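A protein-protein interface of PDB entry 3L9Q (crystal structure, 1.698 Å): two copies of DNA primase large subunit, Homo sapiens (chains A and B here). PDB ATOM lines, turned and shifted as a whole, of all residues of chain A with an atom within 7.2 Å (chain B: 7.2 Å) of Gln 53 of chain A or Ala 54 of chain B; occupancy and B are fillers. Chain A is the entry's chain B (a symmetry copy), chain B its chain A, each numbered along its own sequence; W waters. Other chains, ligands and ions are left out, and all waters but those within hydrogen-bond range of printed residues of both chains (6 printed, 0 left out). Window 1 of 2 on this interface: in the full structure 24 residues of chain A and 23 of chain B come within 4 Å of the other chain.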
ATOM      1  N   HIS A  30      -7.382  13.307  -1.164  1.00  0.00           N
ATOM      2  CA  HIS A  30      -8.308  13.956  -2.089  1.00  0.00           C
ATOM      3  C   HIS A  30      -8.256  15.478  -2.013  1.00  0.00           C
ATOM      4  O   HIS A  30      -9.206  16.167  -2.384  1.00  0.00           O
ATOM      5  CB  HIS A  30      -9.733  13.435  -1.880  1.00  0.00           C
ATOM      6  CG  HIS A  30      -9.857  11.958  -2.080  1.00  0.00           C
ATOM      7  ND1 HIS A  30      -9.763  11.055  -1.044  1.00  0.00           N
ATOM      8  CD2 HIS A  30     -10.039  11.223  -3.204  1.00  0.00           C
ATOM      9  CE1 HIS A  30      -9.891   9.828  -1.518  1.00  0.00           C
ATOM     10  NE2 HIS A  30     -10.060   9.902  -2.826  1.00  0.00           N
ATOM     11  N   HIS A  31      -7.133  15.997  -1.540  1.00  0.00           N
ATOM     12  CA  HIS A  31      -6.930  17.432  -1.437  1.00  0.00           C
ATOM     13  C   HIS A  31      -5.473  17.701  -1.077  1.00  0.00           C
ATOM     14  O   HIS A  31      -4.814  16.851  -0.478  1.00  0.00           O
ATOM     15  CB  HIS A  31      -7.842  18.017  -0.358  1.00  0.00           C
ATOM     16  CG  HIS A  31      -7.680  19.495  -0.161  1.00  0.00           C
ATOM     17  ND1 HIS A  31      -7.108  20.037   0.970  1.00  0.00           N
ATOM     18  CD2 HIS A  31      -8.017  20.542  -0.952  1.00  0.00           C
ATOM     19  CE1 HIS A  31      -7.101  21.356   0.869  1.00  0.00           C
ATOM     20  NE2 HIS A  31      -7.648  21.687  -0.288  1.00  0.00           N
ATOM     21  N   ARG A  37      -0.367  22.138  -3.608  1.00  0.00           N
ATOM     22  CA  ARG A  37      -0.944  22.327  -4.941  1.00  0.00           C
ATOM     23  C   ARG A  37       0.025  23.083  -5.844  1.00  0.00           C
ATOM     24  O   ARG A  37       0.161  22.765  -7.022  1.00  0.00           O
ATOM     25  CB  ARG A  37      -2.293  23.058  -4.880  1.00  0.00           C
ATOM     26  CG  ARG A  37      -3.383  22.250  -4.210  1.00  0.00           C
ATOM     27  CD  ARG A  37      -4.789  22.750  -4.566  1.00  0.00           C
ATOM     28  NE  ARG A  37      -4.952  24.193  -4.367  1.00  0.00           N
ATOM     29  CZ  ARG A  37      -5.296  24.755  -3.210  1.00  0.00           C
ATOM     30  NH1 ARG A  37      -5.501  24.001  -2.134  1.00  0.00           N
ATOM     31  NH2 ARG A  37      -5.427  26.071  -3.120  1.00  0.00           N
ATOM     32  N   THR A  50      -1.745  19.530 -16.891  1.00  0.00           N
ATOM     33  CA  THR A  50      -2.481  20.470 -16.061  1.00  0.00           C
ATOM     34  C   THR A  50      -3.281  19.737 -14.995  1.00  0.00           C
ATOM     35  O   THR A  50      -4.126  18.891 -15.308  1.00  0.00           O
ATOM     36  CB  THR A  50      -3.453  21.311 -16.907  1.00  0.00           C
ATOM     37  OG1 THR A  50      -2.706  22.142 -17.804  1.00  0.00           O
ATOM     38  CG2 THR A  50      -4.327  22.189 -16.010  1.00  0.00           C
ATOM     39  N   LEU A  51      -3.013  20.080 -13.738  1.00  0.00           N
ATOM     40  CA  LEU A  51      -3.736  19.538 -12.597  1.00  0.00           C
ATOM     41  C   LEU A  51      -4.911  20.455 -12.282  1.00  0.00           C
ATOM     42  O   LEU A  51      -4.739  21.663 -12.096  1.00  0.00           O
ATOM     43  CB  LEU A  51      -2.801  19.448 -11.384  1.00  0.00           C
ATOM     44  CG  LEU A  51      -3.438  18.976 -10.074  1.00  0.00           C
ATOM     45  CD1 LEU A  51      -3.840  17.501 -10.165  1.00  0.00           C
ATOM     46  CD2 LEU A  51      -2.487  19.201  -8.901  1.00  0.00           C
ATOM     47  N   GLU A  52      -6.112  19.890 -12.234  1.00  0.00           N
ATOM     48  CA  GLU A  52      -7.293  20.695 -11.974  1.00  0.00           C
ATOM     49  C   GLU A  52      -8.391  19.879 -11.310  1.00  0.00           C
ATOM     50  O   GLU A  52      -8.375  18.657 -11.344  1.00  0.00           O
ATOM     51  CB  GLU A  52      -7.810  21.330 -13.274  1.00  0.00           C
ATOM     52  CG  GLU A  52      -8.250  20.336 -14.334  1.00  0.00           C
ATOM     53  CD  GLU A  52      -8.687  21.027 -15.621  1.00  0.00           C
ATOM     54  OE1 GLU A  52      -8.402  22.237 -15.781  1.00  0.00           O
ATOM     55  OE2 GLU A  52      -9.308  20.363 -16.479  1.00  0.00           O
ATOM     56  N   GLN A  53      -9.348  20.569 -10.705  1.00  0.00           N
ATOM     57  CA  GLN A  53     -10.457  19.911 -10.036  1.00  0.00           C
ATOM     58  C   GLN A  53     -11.707  20.064 -10.895  1.00  0.00           C
ATOM     59  O   GLN A  53     -12.058  21.172 -11.288  1.00  0.00           O
ATOM     60  CB  GLN A  53     -10.658  20.539  -8.654  1.00  0.00           C
ATOM     61  CG  GLN A  53     -11.719  19.885  -7.795  1.00  0.00           C
ATOM     62  CD  GLN A  53     -11.773  20.485  -6.398  1.00  0.00           C
ATOM     63  OE1 GLN A  53     -12.838  20.557  -5.780  1.00  0.00           O
ATOM     64  NE2 GLN A  53     -10.623  20.924  -5.896  1.00  0.00           N
ATOM     65  N   ALA A  54     -12.359  18.947 -11.208  1.00  0.00           N
ATOM     66  CA  ALA A  54     -13.556  18.971 -12.043  1.00  0.00           C
ATOM     67  C   ALA A  54     -14.757  19.449 -11.245  1.00  0.00           C
ATOM     68  O   ALA A  54     -15.001  18.973 -10.139  1.00  0.00           O
ATOM     69  CB  ALA A  54     -13.825  17.595 -12.625  1.00  0.00           C
ATOM     70  N   LEU A  55     -15.497  20.399 -11.810  1.00  0.00           N
ATOM     71  CA  LEU A  55     -16.711  20.915 -11.186  1.00  0.00           C
ATOM     72  C   LEU A  55     -17.908  20.614 -12.069  1.00  0.00           C
ATOM     73  O   LEU A  55     -17.762  20.094 -13.176  1.00  0.00           O
ATOM     74  CB  LEU A  55     -16.612  22.430 -10.967  1.00  0.00           C
ATOM     75  CG  LEU A  55     -15.789  22.943  -9.779  1.00  0.00           C
ATOM     76  CD1 LEU A  55     -14.492  22.199  -9.618  1.00  0.00           C
ATOM     77  CD2 LEU A  55     -15.535  24.443  -9.905  1.00  0.00           C
ATOM     78  N   GLN A  56     -19.092  20.949 -11.577  1.00  0.00           N
ATOM     79  CA  GLN A  56     -20.325  20.746 -12.329  1.00  0.00           C
ATOM     80  C   GLN A  56     -20.951  22.088 -12.708  1.00  0.00           C
ATOM     81  O   GLN A  56     -21.454  22.812 -11.843  1.00  0.00           O
ATOM     82  CB  GLN A  56     -21.300  19.919 -11.495  1.00  0.00           C
ATOM     83  CG  GLN A  56     -20.746  18.551 -11.105  1.00  0.00           C
ATOM     84  CD  GLN A  56     -21.638  17.815 -10.129  1.00  0.00           C
ATOM     85  OE1 GLN A  56     -21.992  18.343  -9.076  1.00  0.00           O
ATOM     86  NE2 GLN A  56     -22.002  16.586 -10.471  1.00  0.00           N
ATOM     87  N   SER A  77     -13.052  16.171  -7.193  1.00  0.00           N
ATOM     88  CA  SER A  77     -12.221  15.187  -7.884  1.00  0.00           C
ATOM     89  C   SER A  77     -11.147  15.830  -8.765  1.00  0.00           C
ATOM     90  O   SER A  77     -11.434  16.677  -9.611  1.00  0.00           O
ATOM     91  CB  SER A  77     -13.085  14.235  -8.716  1.00  0.00           C
ATOM     92  OG  SER A  77     -12.282  13.305  -9.419  1.00  0.00           O
ATOM     93  N   TYR A  78      -9.904  15.410  -8.563  1.00  0.00           N
ATOM     94  CA  TYR A  78      -8.780  15.971  -9.302  1.00  0.00           C
ATOM     95  C   TYR A  78      -8.491  15.229 -10.609  1.00  0.00           C
ATOM     96  O   TYR A  78      -8.503  13.998 -10.659  1.00  0.00           O
ATOM     97  CB  TYR A  78      -7.533  16.012  -8.420  1.00  0.00           C
ATOM     98  CG  TYR A  78      -7.529  17.147  -7.418  1.00  0.00           C
ATOM     99  CD1 TYR A  78      -6.843  18.327  -7.684  1.00  0.00           C
ATOM    100  CD2 TYR A  78      -8.208  17.040  -6.205  1.00  0.00           C
ATOM    101  CE1 TYR A  78      -6.829  19.369  -6.773  1.00  0.00           C
ATOM    102  CE2 TYR A  78      -8.204  18.081  -5.287  1.00  0.00           C
ATOM    103  CZ  TYR A  78      -7.507  19.243  -5.579  1.00  0.00           C
ATOM    104  OH  TYR A  78      -7.482  20.285  -4.677  1.00  0.00           O
ATOM    105  N   ASN A  79      -8.230  15.996 -11.661  1.00  0.00           N
ATOM    106  CA  ASN A  79      -7.922  15.457 -12.979  1.00  0.00           C
ATOM    107  C   ASN A  79      -6.572  15.945 -13.481  1.00  0.00           C
ATOM    108  O   ASN A  79      -6.088  16.997 -13.070  1.00  0.00           O
ATOM    109  CB  ASN A  79      -8.975  15.901 -13.993  1.00  0.00           C
ATOM    110  CG  ASN A  79     -10.233  15.066 -13.941  1.00  0.00           C
ATOM    111  OD1 ASN A  79     -10.225  13.926 -13.474  1.00  0.00           O
ATOM    112  ND2 ASN A  79     -11.329  15.630 -14.440  1.00  0.00           N
ATOM    113  N   ARG A  81      -4.695  16.594 -17.375  1.00  0.00           N
ATOM    114  CA  ARG A  81      -4.860  16.578 -18.813  1.00  0.00           C
ATOM    115  C   ARG A  81      -3.662  17.237 -19.457  1.00  0.00           C
ATOM    116  O   ARG A  81      -2.911  17.961 -18.798  1.00  0.00           O
ATOM    117  CB  ARG A  81      -6.143  17.297 -19.215  1.00  0.00           C
ATOM    118  CG  ARG A  81      -6.256  18.708 -18.672  1.00  0.00           C
ATOM    119  CD  ARG A  81      -7.449  19.430 -19.287  1.00  0.00           C
ATOM    120  NE  ARG A  81      -7.617  20.767 -18.729  1.00  0.00           N
ATOM    121  CZ  ARG A  81      -6.850  21.810 -19.036  1.00  0.00           C
ATOM    122  NH1 ARG A  81      -5.845  21.670 -19.899  1.00  0.00           N
ATOM    123  NH2 ARG A  81      -7.084  22.990 -18.475  1.00  0.00           N
ATOM    124  N   ARG A  90      -1.972  33.858 -17.408  1.00  0.00           N
ATOM    125  CA  ARG A  90      -2.839  34.085 -16.258  1.00  0.00           C
ATOM    126  C   ARG A  90      -2.089  33.937 -14.942  1.00  0.00           C
ATOM    127  O   ARG A  90      -2.479  34.515 -13.929  1.00  0.00           O
ATOM    128  CB  ARG A  90      -4.038  33.135 -16.281  1.00  0.00           C
ATOM    129  CG  ARG A  90      -5.198  33.627 -17.126  1.00  0.00           C
ATOM    130  CD  ARG A  90      -6.524  33.243 -16.490  1.00  0.00           C
ATOM    131  NE  ARG A  90      -6.917  31.875 -16.803  1.00  0.00           N
ATOM    132  CZ  ARG A  90      -7.871  31.205 -16.165  1.00  0.00           C
ATOM    133  NH1 ARG A  90      -8.159  29.964 -16.528  1.00  0.00           N
ATOM    134  NH2 ARG A  90      -8.529  31.764 -15.158  1.00  0.00           N
ATOM    135  N   HIS B  30     -13.156  34.066 -18.392  1.00  0.00           N
ATOM    136  CA  HIS B  30     -12.770  32.761 -17.866  1.00  0.00           C
ATOM    137  C   HIS B  30     -13.812  32.171 -16.925  1.00  0.00           C
ATOM    138  O   HIS B  30     -13.509  31.272 -16.148  1.00  0.00           O
ATOM    139  CB  HIS B  30     -11.415  32.841 -17.146  1.00  0.00           C
ATOM    140  CG  HIS B  30     -10.319  33.407 -17.990  1.00  0.00           C
ATOM    141  ND1 HIS B  30      -9.871  32.792 -19.139  1.00  0.00           N
ATOM    142  CD2 HIS B  30      -9.575  34.531 -17.848  1.00  0.00           C
ATOM    143  CE1 HIS B  30      -8.903  33.514 -19.673  1.00  0.00           C
ATOM    144  NE2 HIS B  30      -8.704  34.574 -18.909  1.00  0.00           N
ATOM    145  N   GLU B  52     -17.150  21.465 -19.667  1.00  0.00           N
ATOM    146  CA  GLU B  52     -16.728  21.156 -18.310  1.00  0.00           C
ATOM    147  C   GLU B  52     -16.068  22.349 -17.648  1.00  0.00           C
ATOM    148  O   GLU B  52     -15.169  22.970 -18.213  1.00  0.00           O
ATOM    149  CB  GLU B  52     -15.789  19.956 -18.254  1.00  0.00           C
ATOM    150  CG  GLU B  52     -15.361  19.649 -16.816  1.00  0.00           C
ATOM    151  CD  GLU B  52     -14.426  18.470 -16.725  1.00  0.00           C
ATOM    152  OE1 GLU B  52     -13.208  18.664 -16.913  1.00  0.00           O
ATOM    153  OE2 GLU B  52     -14.912  17.352 -16.454  1.00  0.00           O
ATOM    154  N   GLN B  53     -16.533  22.656 -16.443  1.00  0.00           N
ATOM    155  CA  GLN B  53     -15.946  23.691 -15.610  1.00  0.00           C
ATOM    156  C   GLN B  53     -14.941  23.016 -14.688  1.00  0.00           C
ATOM    157  O   GLN B  53     -15.234  21.964 -14.128  1.00  0.00           O
ATOM    158  CB  GLN B  53     -17.051  24.362 -14.787  1.00  0.00           C
ATOM    159  CG  GLN B  53     -16.565  25.474 -13.876  1.00  0.00           C
ATOM    160  CD  GLN B  53     -17.638  25.960 -12.917  1.00  0.00           C
ATOM    161  OE1 GLN B  53     -18.728  25.390 -12.838  1.00  0.00           O
ATOM    162  NE2 GLN B  53     -17.325  27.008 -12.169  1.00  0.00           N
ATOM    163  N   ALA B  54     -13.751  23.596 -14.549  1.00  0.00           N
ATOM    164  CA  ALA B  54     -12.742  23.034 -13.654  1.00  0.00           C
ATOM    165  C   ALA B  54     -12.052  24.137 -12.868  1.00  0.00           C
ATOM    166  O   ALA B  54     -12.007  25.279 -13.312  1.00  0.00           O
ATOM    167  CB  ALA B  54     -11.713  22.211 -14.442  1.00  0.00           C
ATOM    168  N   LEU B  55     -11.524  23.787 -11.698  1.00  0.00           N
ATOM    169  CA  LEU B  55     -10.802  24.731 -10.857  1.00  0.00           C
ATOM    170  C   LEU B  55      -9.303  24.428 -10.929  1.00  0.00           C
ATOM    171  O   LEU B  55      -8.877  23.313 -10.638  1.00  0.00           O
ATOM    172  CB  LEU B  55     -11.286  24.616  -9.409  1.00  0.00           C
ATOM    173  CG  LEU B  55     -10.552  25.474  -8.379  1.00  0.00           C
ATOM    174  CD1 LEU B  55     -10.831  26.948  -8.634  1.00  0.00           C
ATOM    175  CD2 LEU B  55     -10.952  25.089  -6.952  1.00  0.00           C
ATOM    176  N   GLN B  56      -8.511  25.424 -11.320  1.00  0.00           N
ATOM    177  CA  GLN B  56      -7.071  25.249 -11.502  1.00  0.00           C
ATOM    178  C   GLN B  56      -6.363  25.145 -10.161  1.00  0.00           C
ATOM    179  O   GLN B  56      -6.804  25.742  -9.183  1.00  0.00           O
ATOM    180  CB  GLN B  56      -6.505  26.417 -12.304  1.00  0.00           C
ATOM    181  CG  GLN B  56      -7.129  26.557 -13.687  1.00  0.00           C
ATOM    182  CD  GLN B  56      -6.568  25.543 -14.675  1.00  0.00           C
ATOM    183  OE1 GLN B  56      -6.953  24.373 -14.674  1.00  0.00           O
ATOM    184  NE2 GLN B  56      -5.658  25.994 -15.526  1.00  0.00           N
ATOM    185  N   PHE B  57      -5.261  24.401 -10.124  1.00  0.00           N
ATOM    186  CA  PHE B  57      -4.566  24.110  -8.869  1.00  0.00           C
ATOM    187  C   PHE B  57      -4.069  25.355  -8.145  1.00  0.00           C
ATOM    188  O   PHE B  57      -3.897  25.339  -6.924  1.00  0.00           O
ATOM    189  CB  PHE B  57      -3.380  23.173  -9.111  1.00  0.00           C
ATOM    190  CG  PHE B  57      -2.245  23.806  -9.881  1.00  0.00           C
ATOM    191  CD1 PHE B  57      -1.289  24.577  -9.232  1.00  0.00           C
ATOM    192  CD2 PHE B  57      -2.129  23.615 -11.251  1.00  0.00           C
ATOM    193  CE1 PHE B  57      -0.235  25.148  -9.936  1.00  0.00           C
ATOM    194  CE2 PHE B  57      -1.082  24.184 -11.966  1.00  0.00           C
ATOM    195  CZ  PHE B  57      -0.131  24.954 -11.308  1.00  0.00           C
ATOM    196  N   LYS B  74     -10.996  34.078 -10.708  1.00  0.00           N
ATOM    197  CA  LYS B  74     -11.648  33.032  -9.922  1.00  0.00           C
ATOM    198  C   LYS B  74     -10.975  31.663 -10.050  1.00  0.00           C
ATOM    199  O   LYS B  74     -11.299  30.740  -9.299  1.00  0.00           O
ATOM    200  CB  LYS B  74     -13.134  32.933 -10.280  1.00  0.00           C
ATOM    201  CG  LYS B  74     -13.917  34.197  -9.970  1.00  0.00           C
ATOM    202  CD  LYS B  74     -15.409  33.974 -10.111  1.00  0.00           C
ATOM    203  CE  LYS B  74     -16.177  35.235  -9.756  1.00  0.00           C
ATOM    204  NZ  LYS B  74     -15.746  36.396 -10.588  1.00  0.00           N
ATOM    205  N   GLY B  75     -10.051  31.541 -11.006  1.00  0.00           N
ATOM    206  CA  GLY B  75      -9.213  30.358 -11.145  1.00  0.00           C
ATOM    207  C   GLY B  75      -9.847  29.190 -11.879  1.00  0.00           C
ATOM    208  O   GLY B  75      -9.442  28.036 -11.703  1.00  0.00           O
ATOM    209  N   TYR B  76     -10.829  29.482 -12.725  1.00  0.00           N
ATOM    210  CA  TYR B  76     -11.519  28.436 -13.469  1.00  0.00           C
ATOM    211  C   TYR B  76     -10.932  28.267 -14.856  1.00  0.00           C
ATOM    212  O   TYR B  76     -10.383  29.206 -15.435  1.00  0.00           O
ATOM    213  CB  TYR B  76     -13.017  28.741 -13.606  1.00  0.00           C
ATOM    214  CG  TYR B  76     -13.757  28.816 -12.294  1.00  0.00           C
ATOM    215  CD1 TYR B  76     -13.869  27.702 -11.474  1.00  0.00           C
ATOM    216  CD2 TYR B  76     -14.348  30.000 -11.874  1.00  0.00           C
ATOM    217  CE1 TYR B  76     -14.543  27.765 -10.268  1.00  0.00           C
ATOM    218  CE2 TYR B  76     -15.033  30.069 -10.674  1.00  0.00           C
ATOM    219  CZ  TYR B  76     -15.126  28.947  -9.876  1.00  0.00           C
ATOM    220  OH  TYR B  76     -15.800  29.006  -8.677  1.00  0.00           O
ATOM    221  N   SER B  77     -11.060  27.055 -15.381  1.00  0.00           N
ATOM    222  CA  SER B  77     -10.695  26.752 -16.748  1.00  0.00           C
ATOM    223  C   SER B  77     -11.836  25.906 -17.296  1.00  0.00           C
ATOM    224  O   SER B  77     -12.344  25.026 -16.605  1.00  0.00           O
ATOM    225  CB  SER B  77      -9.371  25.975 -16.775  1.00  0.00           C
ATOM    226  OG  SER B  77      -8.988  25.664 -18.105  1.00  0.00           O
ATOM    227  N   TYR B  78     -12.277  26.196 -18.514  1.00  0.00           N
ATOM    228  CA  TYR B  78     -13.357  25.429 -19.103  1.00  0.00           C
ATOM    229  C   TYR B  78     -12.821  24.640 -20.281  1.00  0.00           C
ATOM    230  O   TYR B  78     -11.885  25.082 -20.953  1.00  0.00           O
ATOM    231  CB  TYR B  78     -14.477  26.359 -19.565  1.00  0.00           C
ATOM    232  CG  TYR B  78     -15.317  26.927 -18.446  1.00  0.00           C
ATOM    233  CD1 TYR B  78     -16.639  26.526 -18.279  1.00  0.00           C
ATOM    234  CD2 TYR B  78     -14.798  27.875 -17.562  1.00  0.00           C
ATOM    235  CE1 TYR B  78     -17.432  27.056 -17.262  1.00  0.00           C
ATOM    236  CE2 TYR B  78     -15.584  28.409 -16.541  1.00  0.00           C
ATOM    237  CZ  TYR B  78     -16.900  27.992 -16.397  1.00  0.00           C
ATOM    238  OH  TYR B  78     -17.696  28.505 -15.393  1.00  0.00           O
ATOM    239  N   ASN B  79     -13.391  23.463 -20.509  1.00  0.00           N
ATOM    240  CA  ASN B  79     -13.040  22.665 -21.676  1.00  0.00           C
ATOM    241  C   ASN B  79     -14.281  22.025 -22.279  1.00  0.00           C
ATOM    242  O   ASN B  79     -15.342  21.991 -21.649  1.00  0.00           O
ATOM    243  CB  ASN B  79     -11.983  21.601 -21.331  1.00  0.00           C
ATOM    244  CG  ASN B  79     -12.505  20.529 -20.381  1.00  0.00           C
ATOM    245  OD1 ASN B  79     -13.263  19.642 -20.779  1.00  0.00           O
ATOM    246  ND2 ASN B  79     -12.083  20.595 -19.124  1.00  0.00           N
HETATM  247  O   HOH W   1     -10.736  22.679 -18.051  1.00  0.00           O
HETATM  248  O   HOH W   2     -10.906  18.521 -15.701  1.00  0.00           O
HETATM  249  O   HOH W   3     -18.880  20.914 -15.500  1.00  0.00           O
HETATM  250  O   HOH W   4      -7.382  25.494  -6.231  1.00  0.00           O
HETATM  251  O   HOH W   5     -13.906  15.217 -15.769  1.00  0.00           O
HETATM  252  O   HOH W   6     -20.417  25.414 -10.702  1.00  0.00           O
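Printed residues of chain B that touch a printed residue of chain A: His 30, Glu 52, Gln 53, Ala 54, Leu 55, Gln 56, Phe 57, Tyr 76, Ser 77 and Asn 79.
Water W5 bridges the side-chain carboxylate of Glu 52 of chain B and the side-chain amide nitrogen of Asn 79 of chain A. Water W2 lies within hydrogen-bond range of OE2 of Glu 52 of chain A (2.6 Å), OE1 of Glu 52 of chain B (2.6 Å) and ND2 of Asn 79 of chain A (3.2 Å). Water W1 lies within hydrogen-bond range of the side-chain amide nitrogen of Asn 79 of chain B, the side-chain carboxylate of Glu 52 of chain A and the backbone carbonyl oxygen of Ser 77 of chain B. Water W3 bridges the backbone carbonyl oxygen (O) of Leu 55 of chain A (2.7 Å) and the backbone NH (N) of Gln 53 of chain B (3.1 Å). Water W6 lies within hydrogen-bond range of the side-chain amide oxygen (OE1) of Gln 53 of chain B (2.7 Å) and the backbone carbonyl oxygen (O) of Gln 56 of chain A (3.0 Å). Water W4 bridges O of Gln 56 of chain B (3.0 Å) and NE of Arg 37 of chain A (3.3 Å).
Glu 52 of chain A touches Leu 55 of chain B, but with the chains exchanged Leu 55 of chain A does not touch Glu 52 of chain B (4.4 Å). Glu 52 of chain A touches Gln 56 of chain B, but with the chains exchanged Gln 56 of chain A does not touch Glu 52 of chain B (6.6 Å). Gln 53 of chain A touches Leu 55 of chain B, and with the chains exchanged Leu 55 of chain A touches Gln 53 of chain B. Gln 56 of chain A touches Gln 53 of chain B, but with the chains exchanged Gln 53 of chain A does not touch Gln 56 of chain B (5.0 Å). Positions printed for both chains: 30, 52, 53, 54, 55, 56, 77, 78 and 79.
The backbone NH of Glu 52 of chain B sits at hydrogen-bond distance from the backbone carbonyl oxygen of Asn 79 of chain B, 2.7 Å away. O of Ser 77 of chain B is in hydrogen-bond range of N of Ala 54 of chain B (2.9 Å). The backbone carbonyl oxygen of Gly 75 of chain B sits at hydrogen-bond distance from the backbone NH of Gln 56 of chain B (2.8 Å). The side-chain carboxylate (OE2) of Glu 52 of chain A lies within salt-bridge range of the guanidinium group (NE) of Arg 81 of chain A (2.8 Å). The side-chain hydroxyl (OH) of Tyr 78 of chain A lies within hydrogen-bond range of the side-chain amide nitrogen (NE2) of Gln 53 of chain A, at 3.4 Å. The backbone carbonyl oxygen (O) of Ser 77 of chain A sits at hydrogen-bond distance from the backbone NH (N) of Ala 54 of chain A, at 2.9 Å.
Of the printed residues of chain B, Thr 50 of chain A touches Gln 56. Of chain B, only Ala 54 and Leu 55 come within 4 Å of Gln 53 of chain A. Printed residues of chain B within 4 Å of Gln 56 of chain A: Gln 53. Of the printed residues of chain A, Glu 52 of chain B touches Ala 54. Ala 54 of chain B touches two residues of chain A. The nearest residue of chain A that does not touch Ala 54 of chain B is Leu 55 of chain A (4.2 Å). The nearest printed residue of chain B that does not touch Thr 50 of chain A is Phe 57 of chain B (5.4 Å).
Among the printed residues, merely in contact across the chains: Gln 53 of chain A with Ala 54 of chain B (3.1 Å), Glu 52 of chain A with Leu 55 of chain B (3.3 Å), Glu 52 of chain A with Ala 54 of chain B (3.5 Å), Leu 55 of chain A with Tyr 76 of chain B (3.5 Å), Arg 90 of chain A with His 30 of chain B (3.5 Å), Thr 50 of chain A with Gln 56 of chain B (3.7 Å), Glu 52 of chain A with Asn 79 of chain B (3.8 Å), Ala 54 of chain A with Gln 53 of chain B (3.9 Å), Gln 56 of chain A with Gln 53 of chain B (3.9 Å), Leu 55 of chain A with Leu 55 of chain B (3.96 Å), Glu 52 of chain A with Ser 77 of chain B (3.99 Å) and Ala 54 of chain A with Glu 52 of chain B (3.99 Å).
The backbone NH (N) of Leu 55 of chain A is in hydrogen-bond range of the backbone carbonyl oxygen (O) of Gln 53 of chain B, 2.8 Å away. The backbone carbonyl oxygen of Gln 53 of chain A is in hydrogen-bond range of the backbone NH of Leu 55 of chain B, 2.7 Å away. OE1 of Gln 56 of chain B lies close to OE1 of Glu 52 of chain A, 2.8 Å away. The backbone carbonyl oxygen (O) of Phe 57 of chain B lies within hydrogen-bond range of the guanidinium group (NE) of Arg 37 of chain A (3.0 Å). The backbone NH (N) of Phe 57 of chain B lies close to the backbone carbonyl oxygen (O) of Leu 51 of chain A, at 3.4 Å. O of Tyr 76 of chain B is in hydrogen-bond range of NH1 of Arg 90 of chain A, 2.6 Å away. The side-chain hydroxyl of Ser 77 of chain B lies within hydrogen-bond range of the guanidinium group of Arg 81 of chain A, 3.3 Å away.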
